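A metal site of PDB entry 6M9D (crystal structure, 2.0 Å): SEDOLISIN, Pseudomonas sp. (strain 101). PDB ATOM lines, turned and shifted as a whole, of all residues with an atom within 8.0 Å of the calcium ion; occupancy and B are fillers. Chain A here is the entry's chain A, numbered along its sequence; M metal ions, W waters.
The side-chain hydroxyl of Thr 349 is in hydrogen-bond range of the side-chain carboxylate of Asp 346 (2.6 Å).
Within 4 Å of the calcium ion: Asp 326, Val 327, Gly 342, Gly 344 and Asp 346.
The nearest printed residue that does not touch the calcium ion is Thr 343 (4.2 Å).
The side-chain carboxylate (OD1) of Asp 326 is bound to the calcium ion, 2.2 Å away.
The backbone carbonyl oxygen (O) of Val 327 binds the calcium ion, at 2.3 Å.
The backbone carbonyl oxygen (O) of Gly 342 is bound to the calcium ion (2.3 Å).
OD2 of Asp 346 is bound to the calcium ion (2.3 Å).
The backbone carbonyl oxygen (O) of Gly 344 is bound to the calcium ion, 2.4 Å away.
Water W1 binds the calcium ion (2.6 Å).
The calcium ion has six donor atoms within binding distance.
Water W1 lies within hydrogen-bond range of the side-chain hydroxyl of Thr 349 (2.6 Å), the backbone carbonyl oxygen of Gly 350 (2.6 Å) and the backbone NH of Gly 352 (3.5 Å).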
ATOM      1  N   VAL A 217     -20.507   0.619  30.854  1.00  0.00           N
ATOM      2  CA  VAL A 217     -21.924   0.427  31.182  1.00  0.00           C
ATOM      3  C   VAL A 217     -22.342   1.128  32.466  1.00  0.00           C
ATOM      4  O   VAL A 217     -21.571   1.159  33.437  1.00  0.00           O
ATOM      5  CB  VAL A 217     -22.201  -1.086  31.353  1.00  0.00           C
ATOM      6  CG1 VAL A 217     -23.644  -1.300  31.793  1.00  0.00           C
ATOM      7  CG2 VAL A 217     -21.883  -1.841  30.064  1.00  0.00           C
ATOM      8  N   VAL A 324     -20.709   6.307  16.134  1.00  0.00           N
ATOM      9  CA  VAL A 324     -21.048   6.139  17.547  1.00  0.00           C
ATOM     10  C   VAL A 324     -19.834   5.945  18.437  1.00  0.00           C
ATOM     11  O   VAL A 324     -18.749   5.654  17.928  1.00  0.00           O
ATOM     12  CB  VAL A 324     -21.986   4.931  17.736  1.00  0.00           C
ATOM     13  CG1 VAL A 324     -23.308   5.176  17.009  1.00  0.00           C
ATOM     14  CG2 VAL A 324     -21.356   3.645  17.241  1.00  0.00           C
ATOM     15  N   HIS A 325     -20.009   6.074  19.751  1.00  0.00           N
ATOM     16  CA  HIS A 325     -19.033   5.604  20.733  1.00  0.00           C
ATOM     17  C   HIS A 325     -19.395   4.195  21.209  1.00  0.00           C
ATOM     18  O   HIS A 325     -20.341   4.034  21.983  1.00  0.00           O
ATOM     19  CB  HIS A 325     -18.945   6.527  21.943  1.00  0.00           C
ATOM     20  CG  HIS A 325     -18.529   7.921  21.638  1.00  0.00           C
ATOM     21  ND1 HIS A 325     -17.251   8.247  21.241  1.00  0.00           N
ATOM     22  CD2 HIS A 325     -19.208   9.088  21.663  1.00  0.00           C
ATOM     23  CE1 HIS A 325     -17.154   9.545  21.040  1.00  0.00           C
ATOM     24  NE2 HIS A 325     -18.342  10.079  21.285  1.00  0.00           N
ATOM     25  N   ASP A 326     -18.662   3.168  20.786  1.00  0.00           N
ATOM     26  CA  ASP A 326     -19.008   1.791  21.131  1.00  0.00           C
ATOM     27  C   ASP A 326     -18.640   1.445  22.571  1.00  0.00           C
ATOM     28  O   ASP A 326     -17.469   1.329  22.947  1.00  0.00           O
ATOM     29  CB  ASP A 326     -18.318   0.828  20.141  1.00  0.00           C
ATOM     30  CG  ASP A 326     -18.688  -0.629  20.316  1.00  0.00           C
ATOM     31  OD1 ASP A 326     -19.712  -0.941  20.968  1.00  0.00           O
ATOM     32  OD2 ASP A 326     -17.946  -1.485  19.767  1.00  0.00           O
ATOM     33  N   VAL A 327     -19.660   1.232  23.398  1.00  0.00           N
ATOM     34  CA  VAL A 327     -19.414   0.813  24.783  1.00  0.00           C
ATOM     35  C   VAL A 327     -18.935  -0.632  24.775  1.00  0.00           C
ATOM     36  O   VAL A 327     -19.536  -1.478  24.108  1.00  0.00           O
ATOM     37  CB  VAL A 327     -20.664   0.978  25.668  1.00  0.00           C
ATOM     38  CG1 VAL A 327     -20.450   0.359  27.040  1.00  0.00           C
ATOM     39  CG2 VAL A 327     -21.012   2.446  25.811  1.00  0.00           C
ATOM     40  N   LYS A 328     -17.860  -0.936  25.500  1.00  0.00           N
ATOM     41  CA  LYS A 328     -17.283  -2.266  25.485  1.00  0.00           C
ATOM     42  C   LYS A 328     -17.063  -2.872  26.855  1.00  0.00           C
ATOM     43  O   LYS A 328     -16.847  -4.091  26.967  1.00  0.00           O
ATOM     44  CB  LYS A 328     -15.938  -2.223  24.733  1.00  0.00           C
ATOM     45  CG  LYS A 328     -16.078  -1.943  23.239  1.00  0.00           C
ATOM     46  CD  LYS A 328     -14.703  -1.750  22.611  1.00  0.00           C
ATOM     47  CE  LYS A 328     -14.685  -2.036  21.116  1.00  0.00           C
ATOM     48  NZ  LYS A 328     -13.309  -2.335  20.631  1.00  0.00           N
ATOM     49  N   SER A 329     -17.096  -2.095  27.933  1.00  0.00           N
ATOM     50  CA  SER A 329     -16.816  -2.650  29.256  1.00  0.00           C
ATOM     51  C   SER A 329     -17.985  -2.499  30.230  1.00  0.00           C
ATOM     52  O   SER A 329     -18.459  -1.373  30.379  1.00  0.00           O
ATOM     53  CB  SER A 329     -15.580  -1.951  29.845  1.00  0.00           C
ATOM     54  OG  SER A 329     -15.524  -2.136  31.254  1.00  0.00           O
ATOM     55  N   ASN A 340     -23.217  -8.718  29.235  1.00  0.00           N
ATOM     56  CA  ASN A 340     -21.968  -7.994  29.171  1.00  0.00           C
ATOM     57  C   ASN A 340     -21.894  -7.132  27.917  1.00  0.00           C
ATOM     58  O   ASN A 340     -22.375  -7.558  26.865  1.00  0.00           O
ATOM     59  CB  ASN A 340     -20.766  -8.951  29.178  1.00  0.00           C
ATOM     60  CG  ASN A 340     -20.827  -9.812  30.426  1.00  0.00           C
ATOM     61  OD1 ASN A 340     -20.575  -9.306  31.515  1.00  0.00           O
ATOM     62  ND2 ASN A 340     -21.181 -11.081  30.251  1.00  0.00           N
ATOM     63  N   ALA A 341     -21.282  -5.969  28.032  1.00  0.00           N
ATOM     64  CA  ALA A 341     -21.052  -5.146  26.843  1.00  0.00           C
ATOM     65  C   ALA A 341     -20.047  -5.843  25.930  1.00  0.00           C
ATOM     66  O   ALA A 341     -19.323  -6.756  26.346  1.00  0.00           O
ATOM     67  CB  ALA A 341     -20.552  -3.759  27.220  1.00  0.00           C
ATOM     68  N   GLY A 342     -19.955  -5.437  24.675  1.00  0.00           N
ATOM     69  CA  GLY A 342     -18.996  -6.076  23.789  1.00  0.00           C
ATOM     70  C   GLY A 342     -18.843  -5.272  22.512  1.00  0.00           C
ATOM     71  O   GLY A 342     -19.424  -4.184  22.368  1.00  0.00           O
ATOM     72  N   THR A 343     -18.080  -5.826  21.584  1.00  0.00           N
ATOM     73  CA  THR A 343     -17.904  -5.164  20.287  1.00  0.00           C
ATOM     74  C   THR A 343     -19.229  -5.013  19.558  1.00  0.00           C
ATOM     75  O   THR A 343     -20.028  -5.945  19.457  1.00  0.00           O
ATOM     76  CB  THR A 343     -16.892  -5.946  19.431  1.00  0.00           C
ATOM     77  OG1 THR A 343     -15.598  -5.733  20.003  1.00  0.00           O
ATOM     78  CG2 THR A 343     -16.836  -5.389  18.011  1.00  0.00           C
ATOM     79  N   GLY A 344     -19.489  -3.813  19.037  1.00  0.00           N
ATOM     80  CA  GLY A 344     -20.756  -3.540  18.383  1.00  0.00           C
ATOM     81  C   GLY A 344     -21.956  -3.577  19.318  1.00  0.00           C
ATOM     82  O   GLY A 344     -21.857  -3.377  20.527  1.00  0.00           O
ATOM     83  N   TRP A 345     -23.128  -3.829  18.736  1.00  0.00           N
ATOM     84  CA  TRP A 345     -24.371  -3.788  19.483  1.00  0.00           C
ATOM     85  C   TRP A 345     -24.333  -4.723  20.664  1.00  0.00           C
ATOM     86  O   TRP A 345     -23.943  -5.881  20.499  1.00  0.00           O
ATOM     87  CB  TRP A 345     -25.552  -4.170  18.571  1.00  0.00           C
ATOM     88  CG  TRP A 345     -26.869  -3.820  19.194  1.00  0.00           C
ATOM     89  CD1 TRP A 345     -27.585  -2.684  18.945  1.00  0.00           C
ATOM     90  CD2 TRP A 345     -27.623  -4.575  20.145  1.00  0.00           C
ATOM     91  NE1 TRP A 345     -28.736  -2.691  19.682  1.00  0.00           N
ATOM     92  CE2 TRP A 345     -28.798  -3.836  20.427  1.00  0.00           C
ATOM     93  CE3 TRP A 345     -27.449  -5.803  20.799  1.00  0.00           C
ATOM     94  CZ2 TRP A 345     -29.761  -4.278  21.317  1.00  0.00           C
ATOM     95  CZ3 TRP A 345     -28.414  -6.236  21.684  1.00  0.00           C
ATOM     96  CH2 TRP A 345     -29.569  -5.478  21.946  1.00  0.00           C
ATOM     97  N   ASP A 346     -24.747  -4.274  21.854  1.00  0.00           N
ATOM     98  CA  ASP A 346     -24.883  -5.227  22.960  1.00  0.00           C
ATOM     99  C   ASP A 346     -26.150  -4.943  23.770  1.00  0.00           C
ATOM    100  O   ASP A 346     -26.761  -3.888  23.624  1.00  0.00           O
ATOM    101  CB  ASP A 346     -23.650  -5.208  23.853  1.00  0.00           C
ATOM    102  CG  ASP A 346     -23.213  -3.839  24.346  1.00  0.00           C
ATOM    103  OD1 ASP A 346     -23.940  -3.186  25.127  1.00  0.00           O
ATOM    104  OD2 ASP A 346     -22.102  -3.420  23.953  1.00  0.00           O
ATOM    105  N   TYR A 347     -26.535  -5.879  24.635  1.00  0.00           N
ATOM    106  CA  TYR A 347     -27.775  -5.695  25.389  1.00  0.00           C
ATOM    107  C   TYR A 347     -27.722  -4.606  26.442  1.00  0.00           C
ATOM    108  O   TYR A 347     -28.745  -3.952  26.721  1.00  0.00           O
ATOM    109  CB  TYR A 347     -28.160  -7.041  26.030  1.00  0.00           C
ATOM    110  CG  TYR A 347     -28.718  -8.048  25.058  1.00  0.00           C
ATOM    111  CD1 TYR A 347     -27.972  -9.157  24.671  1.00  0.00           C
ATOM    112  CD2 TYR A 347     -29.979  -7.884  24.505  1.00  0.00           C
ATOM    113  CE1 TYR A 347     -28.482 -10.074  23.782  1.00  0.00           C
ATOM    114  CE2 TYR A 347     -30.498  -8.806  23.614  1.00  0.00           C
ATOM    115  CZ  TYR A 347     -29.743  -9.901  23.249  1.00  0.00           C
ATOM    116  OH  TYR A 347     -30.260 -10.817  22.345  1.00  0.00           O
ATOM    117  N   PRO A 348     -26.630  -4.332  27.140  1.00  0.00           N
ATOM    118  CA  PRO A 348     -26.712  -3.195  28.088  1.00  0.00           C
ATOM    119  C   PRO A 348     -26.768  -1.838  27.421  1.00  0.00           C
ATOM    120  O   PRO A 348     -27.375  -0.927  28.003  1.00  0.00           O
ATOM    121  CB  PRO A 348     -25.428  -3.315  28.903  1.00  0.00           C
ATOM    122  CG  PRO A 348     -24.920  -4.709  28.657  1.00  0.00           C
ATOM    123  CD  PRO A 348     -25.317  -5.001  27.224  1.00  0.00           C
ATOM    124  N   THR A 349     -26.152  -1.646  26.247  1.00  0.00           N
ATOM    125  CA  THR A 349     -26.049  -0.287  25.724  1.00  0.00           C
ATOM    126  C   THR A 349     -26.493  -0.126  24.279  1.00  0.00           C
ATOM    127  O   THR A 349     -26.558   1.008  23.770  1.00  0.00           O
ATOM    128  CB  THR A 349     -24.600   0.256  25.854  1.00  0.00           C
ATOM    129  OG1 THR A 349     -23.648  -0.591  25.203  1.00  0.00           O
ATOM    130  CG2 THR A 349     -24.229   0.288  27.334  1.00  0.00           C
ATOM    131  N   GLY A 350     -26.792  -1.230  23.593  1.00  0.00           N
ATOM    132  CA  GLY A 350     -27.131  -1.096  22.173  1.00  0.00           C
ATOM    133  C   GLY A 350     -25.916  -0.685  21.355  1.00  0.00           C
ATOM    134  O   GLY A 350     -24.857  -1.275  21.558  1.00  0.00           O
ATOM    135  N   TRP A 351     -26.058   0.283  20.461  1.00  0.00           N
ATOM    136  CA  TRP A 351     -25.002   0.776  19.598  1.00  0.00           C
ATOM    137  C   TRP A 351     -24.030   1.705  20.340  1.00  0.00           C
ATOM    138  O   TRP A 351     -22.946   1.981  19.835  1.00  0.00           O
ATOM    139  CB  TRP A 351     -25.601   1.523  18.403  1.00  0.00           C
ATOM    140  CG  TRP A 351     -26.243   0.640  17.381  1.00  0.00           C
ATOM    141  CD1 TRP A 351     -27.553   0.665  16.995  1.00  0.00           C
ATOM    142  CD2 TRP A 351     -25.624  -0.403  16.619  1.00  0.00           C
ATOM    143  NE1 TRP A 351     -27.788  -0.288  16.041  1.00  0.00           N
ATOM    144  CE2 TRP A 351     -26.625  -0.970  15.790  1.00  0.00           C
ATOM    145  CE3 TRP A 351     -24.336  -0.927  16.546  1.00  0.00           C
ATOM    146  CZ2 TRP A 351     -26.361  -2.016  14.896  1.00  0.00           C
ATOM    147  CZ3 TRP A 351     -24.058  -1.962  15.666  1.00  0.00           C
ATOM    148  CH2 TRP A 351     -25.077  -2.503  14.854  1.00  0.00           C
ATOM    149  N   GLY A 352     -24.431   2.155  21.524  1.00  0.00           N
ATOM    150  CA  GLY A 352     -23.657   3.125  22.298  1.00  0.00           C
ATOM    151  C   GLY A 352     -24.175   4.539  22.078  1.00  0.00           C
ATOM    152  O   GLY A 352     -25.336   4.713  21.697  1.00  0.00           O
HETATM  153 CA    CA M   1     -20.797  -2.320  22.359  1.00  0.00          CA
HETATM  154  O   HOH W   1     -22.628  -0.555  22.786  1.00  0.00           O
